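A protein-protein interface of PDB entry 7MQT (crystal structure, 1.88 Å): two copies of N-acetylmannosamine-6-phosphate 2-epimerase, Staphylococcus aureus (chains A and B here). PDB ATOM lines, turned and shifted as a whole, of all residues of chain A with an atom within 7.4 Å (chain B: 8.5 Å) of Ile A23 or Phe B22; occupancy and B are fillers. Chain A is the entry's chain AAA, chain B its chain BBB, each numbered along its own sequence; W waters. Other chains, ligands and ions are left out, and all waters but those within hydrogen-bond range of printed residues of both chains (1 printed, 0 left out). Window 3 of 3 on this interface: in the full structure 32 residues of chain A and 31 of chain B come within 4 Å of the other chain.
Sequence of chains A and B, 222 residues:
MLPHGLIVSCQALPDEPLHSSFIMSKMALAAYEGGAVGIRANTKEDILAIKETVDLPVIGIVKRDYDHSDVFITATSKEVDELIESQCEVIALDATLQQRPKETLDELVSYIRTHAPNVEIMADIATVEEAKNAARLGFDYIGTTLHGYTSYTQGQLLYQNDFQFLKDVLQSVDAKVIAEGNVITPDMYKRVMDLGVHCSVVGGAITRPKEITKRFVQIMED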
ATOM      1  N   CYS A  10     -24.069  -2.998  -7.197  1.00  0.00           N
ATOM      2  CA  CYS A  10     -23.213  -3.285  -6.036  1.00  0.00           C
ATOM      3  C   CYS A  10     -23.201  -2.010  -5.211  1.00  0.00           C
ATOM      4  O   CYS A  10     -22.226  -1.237  -5.322  1.00  0.00           O
ATOM      5  CB  CYS A  10     -21.811  -3.712  -6.450  1.00  0.00           C
ATOM      6  SG  CYS A  10     -21.768  -5.245  -7.389  1.00  0.00           S
ATOM      7  N   ALA A  12     -24.096  -0.193  -1.304  1.00  0.00           N
ATOM      8  CA  ALA A  12     -24.304  -0.367   0.138  1.00  0.00           C
ATOM      9  C   ALA A  12     -24.068   1.010   0.720  1.00  0.00           C
ATOM     10  O   ALA A  12     -22.900   1.449   0.730  1.00  0.00           O
ATOM     11  CB  ALA A  12     -23.406  -1.439   0.704  1.00  0.00           C
ATOM     12  N   PRO A  17     -25.016  -3.027   6.122  1.00  0.00           N
ATOM     13  CA  PRO A  17     -23.944  -3.905   6.578  1.00  0.00           C
ATOM     14  C   PRO A  17     -22.690  -3.925   5.694  1.00  0.00           C
ATOM     15  O   PRO A  17     -21.597  -3.965   6.240  1.00  0.00           O
ATOM     16  CB  PRO A  17     -24.610  -5.299   6.559  1.00  0.00           C
ATOM     17  CG  PRO A  17     -26.082  -5.011   6.721  1.00  0.00           C
ATOM     18  CD  PRO A  17     -26.302  -3.717   5.969  1.00  0.00           C
ATOM     19  N   LEU A  18     -22.847  -3.939   4.365  1.00  0.00           N
ATOM     20  CA  LEU A  18     -21.705  -4.151   3.453  1.00  0.00           C
ATOM     21  C   LEU A  18     -21.124  -2.805   3.007  1.00  0.00           C
ATOM     22  O   LEU A  18     -20.279  -2.830   2.140  1.00  0.00           O
ATOM     23  CB  LEU A  18     -22.136  -4.983   2.245  1.00  0.00           C
ATOM     24  CG  LEU A  18     -22.635  -6.391   2.546  1.00  0.00           C
ATOM     25  CD1 LEU A  18     -22.887  -7.133   1.231  1.00  0.00           C
ATOM     26  CD2 LEU A  18     -21.613  -7.143   3.379  1.00  0.00           C
ATOM     27  N   HIS A  19     -21.564  -1.678   3.576  1.00  0.00           N
ATOM     28  CA  HIS A  19     -21.042  -0.328   3.225  1.00  0.00           C
ATOM     29  C   HIS A  19     -19.513  -0.302   3.257  1.00  0.00           C
ATOM     30  O   HIS A  19     -18.901  -0.536   4.322  1.00  0.00           O
ATOM     31  CB  HIS A  19     -21.659   0.751   4.124  1.00  0.00           C
ATOM     32  CG  HIS A  19     -21.092   2.110   3.883  1.00  0.00           C
ATOM     33  ND1 HIS A  19     -21.334   2.816   2.728  1.00  0.00           N
ATOM     34  CD2 HIS A  19     -20.345   2.918   4.661  1.00  0.00           C
ATOM     35  CE1 HIS A  19     -20.720   3.988   2.785  1.00  0.00           C
ATOM     36  NE2 HIS A  19     -20.137   4.078   3.965  1.00  0.00           N
ATOM     37  N   SER A  20     -18.902  -0.027   2.114  1.00  0.00           N
ATOM     38  CA  SER A  20     -17.444  -0.112   1.919  1.00  0.00           C
ATOM     39  C   SER A  20     -17.155  -0.192   0.439  1.00  0.00           C
ATOM     40  O   SER A  20     -17.638  -1.129  -0.188  1.00  0.00           O
ATOM     41  CB  SER A  20     -16.838  -1.327   2.628  1.00  0.00           C
ATOM     42  OG  SER A  20     -15.519  -1.519   2.154  1.00  0.00           O
ATOM     43  N   SER A  21     -16.351   0.736  -0.090  1.00  0.00           N
ATOM     44  CA  SER A  21     -15.849   0.707  -1.474  1.00  0.00           C
ATOM     45  C   SER A  21     -15.189  -0.641  -1.757  1.00  0.00           C
ATOM     46  O   SER A  21     -15.393  -1.229  -2.830  1.00  0.00           O
ATOM     47  CB  SER A  21     -14.878   1.858  -1.710  1.00  0.00           C
ATOM     48  OG  SER A  21     -15.539   3.093  -1.558  1.00  0.00           O
ATOM     49  N   PHE A  22     -14.384  -1.082  -0.799  1.00  0.00           N
ATOM     50  CA  PHE A  22     -13.610  -2.344  -0.825  1.00  0.00           C
ATOM     51  C   PHE A  22     -14.570  -3.515  -1.019  1.00  0.00           C
ATOM     52  O   PHE A  22     -14.401  -4.291  -1.973  1.00  0.00           O
ATOM     53  CB  PHE A  22     -12.830  -2.553   0.477  1.00  0.00           C
ATOM     54  CG  PHE A  22     -12.031  -3.833   0.508  1.00  0.00           C
ATOM     55  CD1 PHE A  22     -10.802  -3.915  -0.130  1.00  0.00           C
ATOM     56  CD2 PHE A  22     -12.521  -4.958   1.140  1.00  0.00           C
ATOM     57  CE1 PHE A  22     -10.072  -5.099  -0.113  1.00  0.00           C
ATOM     58  CE2 PHE A  22     -11.780  -6.128   1.188  1.00  0.00           C
ATOM     59  CZ  PHE A  22     -10.556  -6.193   0.571  1.00  0.00           C
ATOM     60  N   ILE A  23     -15.553  -3.601  -0.143  1.00  0.00           N
ATOM     61  CA  ILE A  23     -16.508  -4.732  -0.163  1.00  0.00           C
ATOM     62  C   ILE A  23     -17.263  -4.687  -1.498  1.00  0.00           C
ATOM     63  O   ILE A  23     -17.377  -5.743  -2.159  1.00  0.00           O
ATOM     64  CB  ILE A  23     -17.397  -4.756   1.064  1.00  0.00           C
ATOM     65  CG1 ILE A  23     -16.548  -4.866   2.331  1.00  0.00           C
ATOM     66  CG2 ILE A  23     -18.436  -5.861   0.965  1.00  0.00           C
ATOM     67  CD1 ILE A  23     -17.380  -4.959   3.576  1.00  0.00           C
ATOM     68  N   MET A  24     -17.687  -3.500  -1.938  1.00  0.00           N
ATOM     69  CA  MET A  24     -18.449  -3.405  -3.206  1.00  0.00           C
ATOM     70  C   MET A  24     -17.563  -3.875  -4.348  1.00  0.00           C
ATOM     71  O   MET A  24     -18.085  -4.608  -5.243  1.00  0.00           O
ATOM     72  CB  MET A  24     -18.989  -1.992  -3.467  1.00  0.00           C
ATOM     73  CG  MET A  24     -20.144  -1.604  -2.555  1.00  0.00           C
ATOM     74  SD  MET A  24     -21.534  -2.745  -2.486  1.00  0.00           S
ATOM     75  CE  MET A  24     -21.192  -3.685  -1.000  1.00  0.00           C
ATOM     76  N   SER A  25     -16.260  -3.588  -4.297  1.00  0.00           N
ATOM     77  CA  SER A  25     -15.312  -4.094  -5.315  1.00  0.00           C
ATOM     78  C   SER A  25     -15.340  -5.625  -5.363  1.00  0.00           C
ATOM     79  O   SER A  25     -15.212  -6.180  -6.437  1.00  0.00           O
ATOM     80  CB  SER A  25     -13.900  -3.554  -5.195  1.00  0.00           C
ATOM     81  OG  SER A  25     -13.235  -4.177  -4.117  1.00  0.00           O
ATOM     82  N   LYS A  26     -15.496  -6.272  -4.215  1.00  0.00           N
ATOM     83  CA  LYS A  26     -15.453  -7.748  -4.082  1.00  0.00           C
ATOM     84  C   LYS A  26     -16.798  -8.311  -4.533  1.00  0.00           C
ATOM     85  O   LYS A  26     -16.791  -9.356  -5.192  1.00  0.00           O
ATOM     86  CB  LYS A  26     -15.032  -8.111  -2.657  1.00  0.00           C
ATOM     87  CG  LYS A  26     -13.587  -7.747  -2.310  1.00  0.00           C
ATOM     88  CD  LYS A  26     -12.616  -8.359  -3.284  1.00  0.00           C
ATOM     89  CE  LYS A  26     -11.140  -8.090  -3.087  1.00  0.00           C
ATOM     90  NZ  LYS A  26     -10.361  -8.822  -4.125  1.00  0.00           N
ATOM     91  N   MET A  27     -17.890  -7.612  -4.223  1.00  0.00           N
ATOM     92  CA  MET A  27     -19.232  -7.973  -4.709  1.00  0.00           C
ATOM     93  C   MET A  27     -19.200  -7.920  -6.233  1.00  0.00           C
ATOM     94  O   MET A  27     -19.779  -8.795  -6.863  1.00  0.00           O
ATOM     95  CB  MET A  27     -20.294  -7.019  -4.162  1.00  0.00           C
ATOM     96  CG  MET A  27     -20.343  -7.029  -2.633  1.00  0.00           C
ATOM     97  SD  MET A  27     -20.836  -8.614  -1.872  1.00  0.00           S
ATOM     98  CE  MET A  27     -22.559  -8.756  -2.292  1.00  0.00           C
ATOM     99  N   ALA A  28     -18.549  -6.915  -6.813  1.00  0.00           N
ATOM    100  CA  ALA A  28     -18.482  -6.756  -8.276  1.00  0.00           C
ATOM    101  C   ALA A  28     -17.653  -7.877  -8.897  1.00  0.00           C
ATOM    102  O   ALA A  28     -18.011  -8.383  -9.977  1.00  0.00           O
ATOM    103  CB  ALA A  28     -17.959  -5.378  -8.631  1.00  0.00           C
ATOM    104  N   LEU A  29     -16.521  -8.218  -8.287  1.00  0.00           N
ATOM    105  CA  LEU A  29     -15.717  -9.366  -8.763  1.00  0.00           C
ATOM    106  C   LEU A  29     -16.586 -10.632  -8.736  1.00  0.00           C
ATOM    107  O   LEU A  29     -16.540 -11.424  -9.671  1.00  0.00           O
ATOM    108  CB  LEU A  29     -14.484  -9.505  -7.877  1.00  0.00           C
ATOM    109  CG  LEU A  29     -13.570 -10.660  -8.230  1.00  0.00           C
ATOM    110  CD1 LEU A  29     -13.013 -10.516  -9.643  1.00  0.00           C
ATOM    111  CD2 LEU A  29     -12.439 -10.747  -7.206  1.00  0.00           C
ATOM    112  N   ASP A  46     -16.552   4.151  -4.722  1.00  0.00           N
ATOM    113  CA  ASP A  46     -16.984   2.749  -4.931  1.00  0.00           C
ATOM    114  C   ASP A  46     -16.652   2.405  -6.374  1.00  0.00           C
ATOM    115  O   ASP A  46     -16.082   1.351  -6.607  1.00  0.00           O
ATOM    116  CB  ASP A  46     -18.455   2.487  -4.629  1.00  0.00           C
ATOM    117  CG  ASP A  46     -18.821   2.454  -3.171  1.00  0.00           C
ATOM    118  OD1 ASP A  46     -18.025   2.999  -2.348  1.00  0.00           O
ATOM    119  OD2 ASP A  46     -19.893   1.878  -2.884  1.00  0.00           O
ATOM    120  N   ALA A  49     -12.854   1.812  -6.844  1.00  0.00           N
ATOM    121  CA  ALA A  49     -12.479   0.532  -6.203  1.00  0.00           C
ATOM    122  C   ALA A  49     -12.930  -0.607  -7.116  1.00  0.00           C
ATOM    123  O   ALA A  49     -12.147  -1.534  -7.397  1.00  0.00           O
ATOM    124  CB  ALA A  49     -13.096   0.439  -4.835  1.00  0.00           C
ATOM    125  N   ILE A  50     -14.172  -0.553  -7.587  1.00  0.00           N
ATOM    126  CA  ILE A  50     -14.722  -1.605  -8.476  1.00  0.00           C
ATOM    127  C   ILE A  50     -13.849  -1.692  -9.732  1.00  0.00           C
ATOM    128  O   ILE A  50     -13.589  -2.798 -10.241  1.00  0.00           O
ATOM    129  CB  ILE A  50     -16.194  -1.325  -8.828  1.00  0.00           C
ATOM    130  CG1 ILE A  50     -17.107  -1.643  -7.654  1.00  0.00           C
ATOM    131  CG2 ILE A  50     -16.582  -2.091 -10.105  1.00  0.00           C
ATOM    132  CD1 ILE A  50     -18.446  -0.928  -7.655  1.00  0.00           C
ATOM    133  N   PRO B  17     -14.368 -14.658  -3.838  1.00  0.00           N
ATOM    134  CA  PRO B  17     -14.232 -13.201  -3.877  1.00  0.00           C
ATOM    135  C   PRO B  17     -14.324 -12.517  -2.503  1.00  0.00           C
ATOM    136  O   PRO B  17     -13.637 -11.533  -2.260  1.00  0.00           O
ATOM    137  CB  PRO B  17     -15.446 -12.760  -4.728  1.00  0.00           C
ATOM    138  CG  PRO B  17     -15.821 -13.967  -5.552  1.00  0.00           C
ATOM    139  CD  PRO B  17     -15.471 -15.153  -4.671  1.00  0.00           C
ATOM    140  N   LEU B  18     -15.180 -13.021  -1.627  1.00  0.00           N
ATOM    141  CA  LEU B  18     -15.524 -12.318  -0.365  1.00  0.00           C
ATOM    142  C   LEU B  18     -14.668 -12.862   0.788  1.00  0.00           C
ATOM    143  O   LEU B  18     -14.939 -12.514   1.909  1.00  0.00           O
ATOM    144  CB  LEU B  18     -17.016 -12.488  -0.075  1.00  0.00           C
ATOM    145  CG  LEU B  18     -17.979 -11.924  -1.121  1.00  0.00           C
ATOM    146  CD1 LEU B  18     -19.382 -11.872  -0.555  1.00  0.00           C
ATOM    147  CD2 LEU B  18     -17.538 -10.532  -1.523  1.00  0.00           C
ATOM    148  N   HIS B  19     -13.647 -13.677   0.524  1.00  0.00           N
ATOM    149  CA  HIS B  19     -12.792 -14.242   1.594  1.00  0.00           C
ATOM    150  C   HIS B  19     -12.301 -13.104   2.509  1.00  0.00           C
ATOM    151  O   HIS B  19     -11.573 -12.185   2.052  1.00  0.00           O
ATOM    152  CB  HIS B  19     -11.622 -15.024   0.980  1.00  0.00           C
ATOM    153  CG  HIS B  19     -10.702 -15.564   2.006  1.00  0.00           C
ATOM    154  ND1 HIS B  19     -11.076 -16.625   2.841  1.00  0.00           N
ATOM    155  CD2 HIS B  19      -9.434 -15.230   2.335  1.00  0.00           C
ATOM    156  CE1 HIS B  19     -10.038 -16.920   3.609  1.00  0.00           C
ATOM    157  NE2 HIS B  19      -9.046 -16.070   3.337  1.00  0.00           N
ATOM    158  N   SER B  20     -12.712 -13.112   3.761  1.00  0.00           N
ATOM    159  CA  SER B  20     -12.436 -12.016   4.720  1.00  0.00           C
ATOM    160  C   SER B  20     -13.273 -12.219   5.968  1.00  0.00           C
ATOM    161  O   SER B  20     -14.514 -12.213   5.820  1.00  0.00           O
ATOM    162  CB  SER B  20     -12.814 -10.650   4.128  1.00  0.00           C
ATOM    163  OG  SER B  20     -12.921  -9.660   5.137  1.00  0.00           O
ATOM    164  N   SER B  21     -12.642 -12.263   7.141  1.00  0.00           N
ATOM    165  CA  SER B  21     -13.347 -12.259   8.441  1.00  0.00           C
ATOM    166  C   SER B  21     -14.263 -11.025   8.549  1.00  0.00           C
ATOM    167  O   SER B  21     -15.400 -11.149   9.025  1.00  0.00           O
ATOM    168  CB  SER B  21     -12.348 -12.366   9.552  1.00  0.00           C
ATOM    169  OG  SER B  21     -11.551 -13.541   9.366  1.00  0.00           O
ATOM    170  N   PHE B  22     -13.814  -9.856   8.084  1.00  0.00           N
ATOM    171  CA  PHE B  22     -14.583  -8.613   8.181  1.00  0.00           C
ATOM    172  C   PHE B  22     -15.823  -8.752   7.294  1.00  0.00           C
ATOM    173  O   PHE B  22     -16.956  -8.506   7.733  1.00  0.00           O
ATOM    174  CB  PHE B  22     -13.689  -7.429   7.788  1.00  0.00           C
ATOM    175  CG  PHE B  22     -14.433  -6.145   7.922  1.00  0.00           C
ATOM    176  CD1 PHE B  22     -14.460  -5.491   9.135  1.00  0.00           C
ATOM    177  CD2 PHE B  22     -15.170  -5.634   6.868  1.00  0.00           C
ATOM    178  CE1 PHE B  22     -15.163  -4.312   9.277  1.00  0.00           C
ATOM    179  CE2 PHE B  22     -15.868  -4.447   7.015  1.00  0.00           C
ATOM    180  CZ  PHE B  22     -15.861  -3.787   8.215  1.00  0.00           C
ATOM    181  N   ILE B  23     -15.654  -9.202   6.062  1.00  0.00           N
ATOM    182  CA  ILE B  23     -16.842  -9.291   5.173  1.00  0.00           C
ATOM    183  C   ILE B  23     -17.804 -10.337   5.735  1.00  0.00           C
ATOM    184  O   ILE B  23     -19.012 -10.100   5.754  1.00  0.00           O
ATOM    185  CB  ILE B  23     -16.475  -9.553   3.718  1.00  0.00           C
ATOM    186  CG1 ILE B  23     -15.563  -8.448   3.175  1.00  0.00           C
ATOM    187  CG2 ILE B  23     -17.744  -9.678   2.907  1.00  0.00           C
ATOM    188  CD1 ILE B  23     -15.111  -8.718   1.754  1.00  0.00           C
ATOM    189  N   MET B  24     -17.313 -11.465   6.196  1.00  0.00           N
ATOM    190  CA  MET B  24     -18.263 -12.492   6.693  1.00  0.00           C
ATOM    191  C   MET B  24     -18.950 -11.962   7.959  1.00  0.00           C
ATOM    192  O   MET B  24     -20.147 -12.282   8.157  1.00  0.00           O
ATOM    193  CB  MET B  24     -17.517 -13.792   6.956  1.00  0.00           C
ATOM    194  CG  MET B  24     -17.079 -14.552   5.716  1.00  0.00           C
ATOM    195  SD  MET B  24     -18.362 -14.813   4.495  1.00  0.00           S
ATOM    196  CE  MET B  24     -18.103 -13.441   3.355  1.00  0.00           C
ATOM    197  N   SER B  25     -18.285 -11.137   8.777  1.00  0.00           N
ATOM    198  CA  SER B  25     -18.939 -10.532   9.968  1.00  0.00           C
ATOM    199  C   SER B  25     -20.117  -9.657   9.510  1.00  0.00           C
ATOM    200  O   SER B  25     -21.124  -9.574  10.232  1.00  0.00           O
ATOM    201  CB  SER B  25     -17.972  -9.801  10.866  1.00  0.00           C
ATOM    202  OG  SER B  25     -17.538  -8.590  10.282  1.00  0.00           O
ATOM    203  N   LYS B  26     -19.966  -8.972   8.369  1.00  0.00           N
ATOM    204  CA  LYS B  26     -21.017  -8.095   7.824  1.00  0.00           C
ATOM    205  C   LYS B  26     -22.128  -8.915   7.172  1.00  0.00           C
ATOM    206  O   LYS B  26     -23.283  -8.486   7.274  1.00  0.00           O
ATOM    207  CB  LYS B  26     -20.425  -7.056   6.869  1.00  0.00           C
ATOM    208  CG  LYS B  26     -19.426  -6.139   7.543  1.00  0.00           C
ATOM    209  CD  LYS B  26     -19.978  -5.523   8.798  1.00  0.00           C
ATOM    210  CE  LYS B  26     -18.991  -4.562   9.388  1.00  0.00           C
ATOM    211  NZ  LYS B  26     -19.577  -3.809  10.511  1.00  0.00           N
ATOM    212  N   MET B  27     -21.800 -10.024   6.506  1.00  0.00           N
ATOM    213  CA  MET B  27     -22.817 -10.954   5.999  1.00  0.00           C
ATOM    214  C   MET B  27     -23.663 -11.435   7.183  1.00  0.00           C
ATOM    215  O   MET B  27     -24.914 -11.464   7.054  1.00  0.00           O
ATOM    216  CB  MET B  27     -22.162 -12.129   5.285  1.00  0.00           C
ATOM    217  CG  MET B  27     -21.601 -11.758   3.952  1.00  0.00           C
ATOM    218  SD  MET B  27     -22.950 -11.402   2.845  1.00  0.00           S
ATOM    219  CE  MET B  27     -22.127 -11.365   1.269  1.00  0.00           C
ATOM    220  N   ALA B  28     -23.010 -11.709   8.312  1.00  0.00           N
ATOM    221  CA  ALA B  28     -23.690 -12.227   9.535  1.00  0.00           C
ATOM    222  C   ALA B  28     -24.581 -11.136  10.120  1.00  0.00           C
ATOM    223  O   ALA B  28     -25.718 -11.428  10.508  1.00  0.00           O
ATOM    224  CB  ALA B  28     -22.682 -12.681  10.540  1.00  0.00           C
ATOM    225  N   LEU B  29     -24.093  -9.896  10.129  1.00  0.00           N
ATOM    226  CA  LEU B  29     -24.884  -8.738  10.587  1.00  0.00           C
ATOM    227  C   LEU B  29     -26.118  -8.638   9.699  1.00  0.00           C
ATOM    228  O   LEU B  29     -27.204  -8.443  10.209  1.00  0.00           O
ATOM    229  CB  LEU B  29     -24.061  -7.451  10.505  1.00  0.00           C
ATOM    230  CG  LEU B  29     -24.778  -6.195  11.013  1.00  0.00           C
ATOM    231  CD1 LEU B  29     -25.239  -6.399  12.444  1.00  0.00           C
ATOM    232  CD2 LEU B  29     -23.872  -4.961  10.923  1.00  0.00           C
ATOM    233  N   GLU B  45     -10.968 -17.306  12.870  1.00  0.00           N
ATOM    234  CA  GLU B  45     -10.822 -15.860  12.552  1.00  0.00           C
ATOM    235  C   GLU B  45     -12.200 -15.282  12.168  1.00  0.00           C
ATOM    236  O   GLU B  45     -12.595 -14.227  12.705  1.00  0.00           O
ATOM    237  CB  GLU B  45      -9.750 -15.694  11.477  1.00  0.00           C
ATOM    238  CG  GLU B  45      -8.337 -15.962  11.989  1.00  0.00           C
ATOM    239  CD  GLU B  45      -7.956 -17.409  12.294  1.00  0.00           C
ATOM    240  OE1 GLU B  45      -8.580 -18.331  11.708  1.00  0.00           O
ATOM    241  OE2 GLU B  45      -7.031 -17.618  13.133  1.00  0.00           O
ATOM    242  N   ASP B  46     -12.926 -15.972  11.292  1.00  0.00           N
ATOM    243  CA  ASP B  46     -14.289 -15.556  10.858  1.00  0.00           C
ATOM    244  C   ASP B  46     -15.227 -15.648  12.042  1.00  0.00           C
ATOM    245  O   ASP B  46     -16.068 -14.755  12.230  1.00  0.00           O
ATOM    246  CB  ASP B  46     -14.808 -16.344   9.665  1.00  0.00           C
ATOM    247  CG  ASP B  46     -14.113 -16.076   8.354  1.00  0.00           C
ATOM    248  OD1 ASP B  46     -13.004 -15.485   8.380  1.00  0.00           O
ATOM    249  OD2 ASP B  46     -14.665 -16.516   7.302  1.00  0.00           O
ATOM    250  N   ILE B  47     -15.155 -16.740  12.788  1.00  0.00           N
ATOM    251  CA  ILE B  47     -16.112 -16.960  13.890  1.00  0.00           C
ATOM    252  C   ILE B  47     -15.937 -15.837  14.924  1.00  0.00           C
ATOM    253  O   ILE B  47     -16.952 -15.310  15.390  1.00  0.00           O
ATOM    254  CB  ILE B  47     -15.922 -18.354  14.493  1.00  0.00           C
ATOM    255  CG1 ILE B  47     -16.300 -19.458  13.506  1.00  0.00           C
ATOM    256  CG2 ILE B  47     -16.710 -18.464  15.768  1.00  0.00           C
ATOM    257  CD1 ILE B  47     -15.816 -20.828  13.919  1.00  0.00           C
ATOM    258  N   ALA B  49     -14.798 -12.817  14.626  1.00  0.00           N
ATOM    259  CA  ALA B  49     -15.226 -11.547  14.018  1.00  0.00           C
ATOM    260  C   ALA B  49     -16.759 -11.495  14.051  1.00  0.00           C
ATOM    261  O   ALA B  49     -17.323 -10.459  14.452  1.00  0.00           O
ATOM    262  CB  ALA B  49     -14.657 -11.436  12.626  1.00  0.00           C
ATOM    263  N   ILE B  50     -17.410 -12.610  13.705  1.00  0.00           N
ATOM    264  CA  ILE B  50     -18.894 -12.708  13.681  1.00  0.00           C
ATOM    265  C   ILE B  50     -19.397 -12.545  15.111  1.00  0.00           C
ATOM    266  O   ILE B  50     -20.376 -11.817  15.326  1.00  0.00           O
ATOM    267  CB  ILE B  50     -19.340 -14.033  13.035  1.00  0.00           C
ATOM    268  CG1 ILE B  50     -19.040 -14.003  11.538  1.00  0.00           C
ATOM    269  CG2 ILE B  50     -20.805 -14.336  13.372  1.00  0.00           C
ATOM    270  CD1 ILE B  50     -19.135 -15.336  10.811  1.00  0.00           C
ATOM    271  N   THR B  53     -19.688  -9.200  16.297  1.00  0.00           N
ATOM    272  CA  THR B  53     -20.628  -8.380  15.487  1.00  0.00           C
ATOM    273  C   THR B  53     -22.072  -8.703  15.883  1.00  0.00           C
ATOM    274  O   THR B  53     -22.897  -7.803  15.880  1.00  0.00           O
ATOM    275  CB  THR B  53     -20.358  -8.641  14.008  1.00  0.00           C
ATOM    276  OG1 THR B  53     -18.978  -8.350  13.828  1.00  0.00           O
ATOM    277  CG2 THR B  53     -21.221  -7.839  13.063  1.00  0.00           C
ATOM    278  N   PRO B 209     -22.747 -13.965  -3.713  1.00  0.00           N
ATOM    279  CA  PRO B 209     -23.267 -13.238  -4.868  1.00  0.00           C
ATOM    280  C   PRO B 209     -22.838 -13.901  -6.189  1.00  0.00           C
ATOM    281  O   PRO B 209     -23.562 -13.820  -7.146  1.00  0.00           O
ATOM    282  CB  PRO B 209     -22.680 -11.825  -4.696  1.00  0.00           C
ATOM    283  CG  PRO B 209     -21.537 -11.992  -3.718  1.00  0.00           C
ATOM    284  CD  PRO B 209     -22.029 -13.088  -2.787  1.00  0.00           C
HETATM  285  O   HOH W   1     -11.224 -11.237  -3.678  1.00  0.00           O
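N of Ile A23 lies within hydrogen-bond range of OG of Ser A20, at 3.1 Å.
The backbone NH of Phe B22 lies within hydrogen-bond range of the side-chain hydroxyl of Ser B20 (3.1 Å).
The side-chain hydroxyl (OG) of Ser B20 sits at hydrogen-bond distance from the backbone NH (N) of Ile B23 (2.9 Å).
The side-chain hydroxyl (OG) of Ser B25 is in hydrogen-bond range of the backbone carbonyl oxygen (O) of Phe B22 (2.6 Å).
CG of Lys B26 touches O of Pro A17, 3.3 Å away.
CB of Lys B26 touches CD2 of Leu A18 (3.7 Å).
Phe B22 touches Ile A23 (CE2 to CD1, 3.8 Å).
Ile B23 touches Ile A23 (CG1 to CG1, 3.8 Å).
Lys A26 touches Pro B17.
CB of Lys A26 touches CD2 of Leu B18, at 3.7 Å.
Met A27 touches Leu B18.
Pro B209 touches Met A27 (CG to CE, 3.7 Å).
Cys A10 touches none of the printed residues of chain B.
Of the printed residues of chain B, Pro A17 touches Lys B26.
Printed residues of chain B within 4 Å of Leu A18: Lys B26.
Ile A23 touches two residues of chain B.
Printed residues of chain B within 4 Å of Met A27: Leu B18 and Pro B209.
His B19 touches none of the printed residues of chain A.
Of the printed residues of chain A, Phe B22 touches Ile A23.
Of the printed residues of chain A, Ile B23 touches Ile A23 (3.8 Å).
The nearest residue of chain B that does not touch Ile A23 is Lys B26 (4.6 Å).
The nearest printed residue of chain B that does not touch Leu A18 is Met B27 (4.3 Å).
Of the 20 printed residues of chain B, 6 touch a printed residue of chain A.
Hydrophobic or aromatic side chains of chain B within 4 Å of the printed part of chain A: Pro B17, Leu B18, Phe B22, Ile B23 and Pro B209.
Of the 18 printed residues of chain A, 5 touch a printed residue of chain B.
Hydrophobic or aromatic side chains of chain A within 4 Å of the printed part of chain B: Pro A17, Leu A18, Ile A23 and Met A27.
Pro A17 touches Lys B26, and with the chains exchanged Lys A26 touches Pro B17.
Leu A18 touches Lys B26, and with the chains exchanged Lys A26 touches Leu B18.
Ile A23 touches Phe B22, but with the chains exchanged Phe A22 does not touch Ile B23 (4.3 Å).
Met A27 touches Leu B18, but with the chains exchanged Leu A18 does not touch Met B27 (4.3 Å).
Positions printed for both chains: 17, 18, 19, 20, 21, 22, 23, 24, 25, 26, 27, 28, 29, 46, 49 and 50.
Of the 8 pairs that touch across the chains among the printed residues, 5 have their exchanged pair printed and touching as well.
Water W1 lies within hydrogen-bond range of NZ of Lys A26 and O of Pro B17.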
